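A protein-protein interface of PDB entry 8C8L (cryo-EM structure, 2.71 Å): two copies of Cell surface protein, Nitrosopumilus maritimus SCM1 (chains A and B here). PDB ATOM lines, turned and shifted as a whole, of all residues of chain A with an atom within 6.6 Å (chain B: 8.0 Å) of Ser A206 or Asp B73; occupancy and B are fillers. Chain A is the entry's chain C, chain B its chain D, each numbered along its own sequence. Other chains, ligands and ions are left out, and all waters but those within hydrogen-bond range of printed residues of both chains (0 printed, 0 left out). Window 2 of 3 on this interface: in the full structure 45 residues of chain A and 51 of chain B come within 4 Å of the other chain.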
ATOM      1  N   ASP A  73       8.666  19.667  13.171  1.00  0.00           N
ATOM      2  CA  ASP A  73       9.755  18.752  12.756  1.00  0.00           C
ATOM      3  C   ASP A  73      11.093  19.278  13.281  1.00  0.00           C
ATOM      4  O   ASP A  73      12.081  18.557  13.153  1.00  0.00           O
ATOM      5  CB  ASP A  73       9.744  18.575  11.243  1.00  0.00           C
ATOM      6  CG  ASP A  73       9.763  19.889  10.481  1.00  0.00           C
ATOM      7  OD1 ASP A  73      10.452  19.955   9.441  1.00  0.00           O
ATOM      8  OD2 ASP A  73       9.083  20.843  10.934  1.00  0.00           O
ATOM      9  N   GLU A  74      11.134  20.482  13.842  1.00  0.00           N
ATOM     10  CA  GLU A  74      12.368  21.034  14.458  1.00  0.00           C
ATOM     11  C   GLU A  74      12.168  21.156  15.968  1.00  0.00           C
ATOM     12  O   GLU A  74      11.015  21.334  16.418  1.00  0.00           O
ATOM     13  CB  GLU A  74      12.714  22.387  13.853  1.00  0.00           C
ATOM     14  CG  GLU A  74      13.354  22.303  12.483  1.00  0.00           C
ATOM     15  CD  GLU A  74      13.746  23.656  11.907  1.00  0.00           C
ATOM     16  OE1 GLU A  74      14.968  23.939  11.824  1.00  0.00           O
ATOM     17  OE2 GLU A  74      12.827  24.429  11.542  1.00  0.00           O
ATOM     18  N   ALA A  75      13.250  21.066  16.730  1.00  0.00           N
ATOM     19  CA  ALA A  75      13.206  21.134  18.204  1.00  0.00           C
ATOM     20  C   ALA A  75      13.294  22.589  18.655  1.00  0.00           C
ATOM     21  O   ALA A  75      14.318  22.980  19.218  1.00  0.00           O
ATOM     22  CB  ALA A  75      14.304  20.303  18.791  1.00  0.00           C
ATOM     23  N   LYS A  76      12.237  23.360  18.467  1.00  0.00           N
ATOM     24  CA  LYS A  76      12.153  24.717  19.063  1.00  0.00           C
ATOM     25  C   LYS A  76      11.975  24.622  20.577  1.00  0.00           C
ATOM     26  O   LYS A  76      11.533  23.582  21.103  1.00  0.00           O
ATOM     27  CB  LYS A  76      11.019  25.523  18.450  1.00  0.00           C
ATOM     28  CG  LYS A  76      11.205  25.807  16.969  1.00  0.00           C
ATOM     29  CD  LYS A  76      12.426  26.667  16.670  1.00  0.00           C
ATOM     30  CE  LYS A  76      12.709  26.827  15.188  1.00  0.00           C
ATOM     31  NZ  LYS A  76      11.479  27.094  14.392  1.00  0.00           N
ATOM     32  N   SER A 204      10.056  12.382  16.021  1.00  0.00           N
ATOM     33  CA  SER A 204      10.774  12.228  14.737  1.00  0.00           C
ATOM     34  C   SER A 204      12.111  12.960  14.832  1.00  0.00           C
ATOM     35  O   SER A 204      12.107  14.166  15.143  1.00  0.00           O
ATOM     36  CB  SER A 204       9.945  12.732  13.586  1.00  0.00           C
ATOM     37  OG  SER A 204       9.751  14.142  13.666  1.00  0.00           O
ATOM     38  N   GLY A 205      13.209  12.261  14.532  1.00  0.00           N
ATOM     39  CA  GLY A 205      14.563  12.839  14.468  1.00  0.00           C
ATOM     40  C   GLY A 205      14.975  13.448  15.797  1.00  0.00           C
ATOM     41  O   GLY A 205      15.025  12.706  16.805  1.00  0.00           O
ATOM     42  N   SER A 206      15.220  14.759  15.817  1.00  0.00           N
ATOM     43  CA  SER A 206      15.637  15.500  17.036  1.00  0.00           C
ATOM     44  C   SER A 206      14.437  15.753  17.963  1.00  0.00           C
ATOM     45  O   SER A 206      14.665  16.071  19.144  1.00  0.00           O
ATOM     46  CB  SER A 206      16.328  16.776  16.670  1.00  0.00           C
ATOM     47  OG  SER A 206      15.461  17.611  15.930  1.00  0.00           O
ATOM     48  N   VAL A 207      13.209  15.595  17.479  1.00  0.00           N
ATOM     49  CA  VAL A 207      11.999  15.996  18.246  1.00  0.00           C
ATOM     50  C   VAL A 207      11.559  14.844  19.157  1.00  0.00           C
ATOM     51  O   VAL A 207      11.429  13.713  18.673  1.00  0.00           O
ATOM     52  CB  VAL A 207      10.876  16.430  17.294  1.00  0.00           C
ATOM     53  CG1 VAL A 207       9.700  16.977  18.047  1.00  0.00           C
ATOM     54  CG2 VAL A 207      11.364  17.439  16.266  1.00  0.00           C
ATOM     55  N   SER A 208      11.339  15.118  20.444  1.00  0.00           N
ATOM     56  CA  SER A 208      10.737  14.161  21.413  1.00  0.00           C
ATOM     57  C   SER A 208       9.199  14.209  21.386  1.00  0.00           C
ATOM     58  O   SER A 208       8.641  15.111  20.767  1.00  0.00           O
ATOM     59  CB  SER A 208      11.239  14.420  22.789  1.00  0.00           C
ATOM     60  OG  SER A 208      10.838  13.354  23.637  1.00  0.00           O
ATOM     61  N   ILE B  69      18.086  32.481  18.065  1.00  0.00           N
ATOM     62  CA  ILE B  69      18.906  31.382  18.652  1.00  0.00           C
ATOM     63  C   ILE B  69      18.025  30.445  19.486  1.00  0.00           C
ATOM     64  O   ILE B  69      18.568  29.609  20.205  1.00  0.00           O
ATOM     65  CB  ILE B  69      20.072  31.990  19.448  1.00  0.00           C
ATOM     66  CG1 ILE B  69      19.574  32.941  20.533  1.00  0.00           C
ATOM     67  CG2 ILE B  69      21.061  32.668  18.517  1.00  0.00           C
ATOM     68  CD1 ILE B  69      20.662  33.493  21.411  1.00  0.00           C
ATOM     69  N   ASN B  70      16.706  30.496  19.314  1.00  0.00           N
ATOM     70  CA  ASN B  70      15.758  29.735  20.177  1.00  0.00           C
ATOM     71  C   ASN B  70      15.742  28.236  19.860  1.00  0.00           C
ATOM     72  O   ASN B  70      15.144  27.492  20.639  1.00  0.00           O
ATOM     73  CB  ASN B  70      14.339  30.282  20.111  1.00  0.00           C
ATOM     74  CG  ASN B  70      13.744  30.202  18.729  1.00  0.00           C
ATOM     75  OD1 ASN B  70      14.298  29.553  17.842  1.00  0.00           O
ATOM     76  ND2 ASN B  70      12.603  30.846  18.541  1.00  0.00           N
ATOM     77  N   ASP B  71      16.359  27.777  18.789  1.00  0.00           N
ATOM     78  CA  ASP B  71      16.321  26.328  18.463  1.00  0.00           C
ATOM     79  C   ASP B  71      17.246  25.548  19.395  1.00  0.00           C
ATOM     80  O   ASP B  71      18.179  26.132  19.947  1.00  0.00           O
ATOM     81  CB  ASP B  71      16.683  26.057  17.006  1.00  0.00           C
ATOM     82  CG  ASP B  71      18.045  26.592  16.619  1.00  0.00           C
ATOM     83  OD1 ASP B  71      18.729  27.152  17.499  1.00  0.00           O
ATOM     84  OD2 ASP B  71      18.404  26.475  15.430  1.00  0.00           O
ATOM     85  N   THR B  72      16.993  24.264  19.565  1.00  0.00           N
ATOM     86  CA  THR B  72      17.722  23.424  20.548  1.00  0.00           C
ATOM     87  C   THR B  72      18.307  22.176  19.891  1.00  0.00           C
ATOM     88  O   THR B  72      18.988  21.423  20.603  1.00  0.00           O
ATOM     89  CB  THR B  72      16.808  23.028  21.710  1.00  0.00           C
ATOM     90  OG1 THR B  72      15.763  22.173  21.248  1.00  0.00           O
ATOM     91  CG2 THR B  72      16.155  24.222  22.362  1.00  0.00           C
ATOM     92  N   ASP B  73      18.061  21.957  18.603  1.00  0.00           N
ATOM     93  CA  ASP B  73      18.605  20.790  17.869  1.00  0.00           C
ATOM     94  C   ASP B  73      19.741  21.251  16.950  1.00  0.00           C
ATOM     95  O   ASP B  73      20.402  20.380  16.369  1.00  0.00           O
ATOM     96  CB  ASP B  73      17.495  20.083  17.101  1.00  0.00           C
ATOM     97  CG  ASP B  73      16.682  21.016  16.215  1.00  0.00           C
ATOM     98  OD1 ASP B  73      16.320  20.595  15.096  1.00  0.00           O
ATOM     99  OD2 ASP B  73      16.413  22.162  16.656  1.00  0.00           O
ATOM    100  N   GLU B  74      19.962  22.557  16.807  1.00  0.00           N
ATOM    101  CA  GLU B  74      21.096  23.086  16.010  1.00  0.00           C
ATOM    102  C   GLU B  74      22.098  23.766  16.940  1.00  0.00           C
ATOM    103  O   GLU B  74      21.688  24.276  18.001  1.00  0.00           O
ATOM    104  CB  GLU B  74      20.599  24.057  14.949  1.00  0.00           C
ATOM    105  CG  GLU B  74      19.988  23.383  13.739  1.00  0.00           C
ATOM    106  CD  GLU B  74      19.541  24.359  12.659  1.00  0.00           C
ATOM    107  OE1 GLU B  74      20.199  24.408  11.587  1.00  0.00           O
ATOM    108  OE2 GLU B  74      18.537  25.077  12.890  1.00  0.00           O
ATOM    109  N   ALA B  75      23.369  23.780  16.558  1.00  0.00           N
ATOM    110  CA  ALA B  75      24.445  24.382  17.369  1.00  0.00           C
ATOM    111  C   ALA B  75      24.568  25.869  17.035  1.00  0.00           C
ATOM    112  O   ALA B  75      25.571  26.259  16.428  1.00  0.00           O
ATOM    113  CB  ALA B  75      25.734  23.655  17.144  1.00  0.00           C
ATOM    114  N   LYS B  76      23.615  26.682  17.465  1.00  0.00           N
ATOM    115  CA  LYS B  76      23.760  28.154  17.367  1.00  0.00           C
ATOM    116  C   LYS B  76      24.816  28.643  18.362  1.00  0.00           C
ATOM    117  O   LYS B  76      25.123  27.942  19.367  1.00  0.00           O
ATOM    118  CB  LYS B  76      22.431  28.855  17.639  1.00  0.00           C
ATOM    119  CG  LYS B  76      21.355  28.540  16.614  1.00  0.00           C
ATOM    120  CD  LYS B  76      21.699  29.039  15.225  1.00  0.00           C
ATOM    121  CE  LYS B  76      20.727  28.634  14.138  1.00  0.00           C
ATOM    122  NZ  LYS B  76      19.314  28.774  14.562  1.00  0.00           N
ATOM    123  N   GLN B  92      22.282  27.068  27.398  1.00  0.00           N
ATOM    124  CA  GLN B  92      20.895  27.066  26.863  1.00  0.00           C
ATOM    125  C   GLN B  92      20.019  26.131  27.680  1.00  0.00           C
ATOM    126  O   GLN B  92      20.532  25.115  28.056  1.00  0.00           O
ATOM    127  CB  GLN B  92      20.760  26.549  25.452  1.00  0.00           C
ATOM    128  CG  GLN B  92      19.565  27.178  24.773  1.00  0.00           C
ATOM    129  CD  GLN B  92      19.406  26.711  23.356  1.00  0.00           C
ATOM    130  OE1 GLN B  92      18.804  27.375  22.517  1.00  0.00           O
ATOM    131  NE2 GLN B  92      19.943  25.543  23.098  1.00  0.00           N
ATOM    132  N   VAL B 201      19.526  21.926  27.954  1.00  0.00           N
ATOM    133  CA  VAL B 201      19.268  21.311  26.617  1.00  0.00           C
ATOM    134  C   VAL B 201      20.110  20.055  26.487  1.00  0.00           C
ATOM    135  O   VAL B 201      21.172  20.070  27.026  1.00  0.00           O
ATOM    136  CB  VAL B 201      19.638  22.354  25.556  1.00  0.00           C
ATOM    137  CG1 VAL B 201      19.583  21.835  24.134  1.00  0.00           C
ATOM    138  CG2 VAL B 201      18.731  23.567  25.705  1.00  0.00           C
ATOM    139  N   ALA B 202      19.647  18.971  25.886  1.00  0.00           N
ATOM    140  CA  ALA B 202      20.401  17.692  25.945  1.00  0.00           C
ATOM    141  C   ALA B 202      21.398  17.581  24.785  1.00  0.00           C
ATOM    142  O   ALA B 202      21.256  18.313  23.797  1.00  0.00           O
ATOM    143  CB  ALA B 202      19.446  16.541  25.950  1.00  0.00           C
ATOM    144  N   SER B 204      22.471  16.075  21.613  1.00  0.00           N
ATOM    145  CA  SER B 204      22.001  15.346  20.415  1.00  0.00           C
ATOM    146  C   SER B 204      22.783  15.832  19.199  1.00  0.00           C
ATOM    147  O   SER B 204      22.783  17.051  18.947  1.00  0.00           O
ATOM    148  CB  SER B 204      20.514  15.517  20.226  1.00  0.00           C
ATOM    149  OG  SER B 204      20.184  16.865  19.915  1.00  0.00           O
ATOM    150  N   GLY B 205      23.393  14.907  18.458  1.00  0.00           N
ATOM    151  CA  GLY B 205      24.102  15.192  17.196  1.00  0.00           C
ATOM    152  C   GLY B 205      25.237  16.179  17.402  1.00  0.00           C
ATOM    153  O   GLY B 205      26.162  15.866  18.176  1.00  0.00           O
ATOM    154  N   SER B 206      25.156  17.346  16.763  1.00  0.00           N
ATOM    155  CA  SER B 206      26.183  18.413  16.857  1.00  0.00           C
ATOM    156  C   SER B 206      26.065  19.177  18.185  1.00  0.00           C
ATOM    157  O   SER B 206      27.030  19.869  18.550  1.00  0.00           O
ATOM    158  CB  SER B 206      26.093  19.337  15.682  1.00  0.00           C
ATOM    159  OG  SER B 206      24.822  19.959  15.640  1.00  0.00           O
ATOM    160  N   VAL B 207      24.954  19.046  18.904  1.00  0.00           N
ATOM    161  CA  VAL B 207      24.687  19.887  20.105  1.00  0.00           C
ATOM    162  C   VAL B 207      25.312  19.229  21.341  1.00  0.00           C
ATOM    163  O   VAL B 207      25.081  18.034  21.570  1.00  0.00           O
ATOM    164  CB  VAL B 207      23.179  20.111  20.281  1.00  0.00           C
ATOM    165  CG1 VAL B 207      22.908  21.084  21.389  1.00  0.00           C
ATOM    166  CG2 VAL B 207      22.518  20.579  18.995  1.00  0.00           C
ATOM    167  N   GLN B 211      24.394  23.355  25.205  1.00  0.00           N
ATOM    168  CA  GLN B 211      24.950  23.959  23.959  1.00  0.00           C
ATOM    169  C   GLN B 211      26.304  24.644  24.201  1.00  0.00           C
ATOM    170  O   GLN B 211      26.792  25.243  23.255  1.00  0.00           O
ATOM    171  CB  GLN B 211      23.927  24.918  23.334  1.00  0.00           C
ATOM    172  CG  GLN B 211      23.935  24.876  21.796  1.00  0.00           C
ATOM    173  CD  GLN B 211      22.610  25.265  21.183  1.00  0.00           C
ATOM    174  OE1 GLN B 211      22.312  26.445  20.971  1.00  0.00           O
ATOM    175  NE2 GLN B 211      21.785  24.276  20.898  1.00  0.00           N
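Of the printed residues of chain B, Ser A206 touches Asp B73.
Printed residues of chain A within 4 Å of Asp B73: Ala A75 and Ser A206.
Ala A75 touches three residues of chain B.
No residue of chain B comes within 4 Å of Gly A205.
Of the printed residues of chain B, Glu A74 touches Glu B74 (3.9 Å).
Printed residues of chain A within 4 Å of Glu B74: Glu A74.
Printed residues of chain A within 4 Å of Asn B70: Lys A76 (3.6 Å).
Printed residues of chain A within 4 Å of Asp B71: Ala A75 (3.9 Å).
The nearest residue of chain A that does not touch Asp B73 is Glu A74 (4.03 Å).
Glu B74 touches its own counterpart, Glu A74.
Ala A75 touches Asp B73, but with the chains exchanged Asp A73 does not touch Ala B75 (12.9 Å).
Ser A206 touches Asp B73, but with the chains exchanged Asp A73 does not touch Ser B206 (13.1 Å).
8 positions are printed for both chains.
The backbone carbonyl oxygen (O) of Glu B74 sits at hydrogen-bond distance from the side-chain amide nitrogen (NE2) of Gln B211 (2.9 Å).
The side-chain carboxylate (OD2) of Asp B71 is in salt-bridge range of the side-chain amino group (NZ) of Lys B76 (2.6 Å).
The side-chain amide oxygen (OE1) of Gln B92 sits close to the backbone carbonyl oxygen (O) of Asp B71, 2.9 Å away.
Among the printed residues, pairs that only touch across the chains: Lys A76 with Asn B70, Glu A74 with Glu B74 and Ala A75 with Asp B71.
Of the 9 printed residues of chain A, 4 touch a printed residue of chain B.
Of the 16 printed residues of chain B, 5 touch a printed residue of chain A.
Among the printed residues, 6 pairs touch across the chains.
The side-chain carboxylate (OD1) of Asp B73 sits at hydrogen-bond distance from the side-chain hydroxyl (OG) of Ser A206.
OD2 of Asp B73 is in hydrogen-bond range of N of Ala A75 (3.3 Å).
OG1 of Thr B72 is in hydrogen-bond range of O of Ala A75 (2.6 Å).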
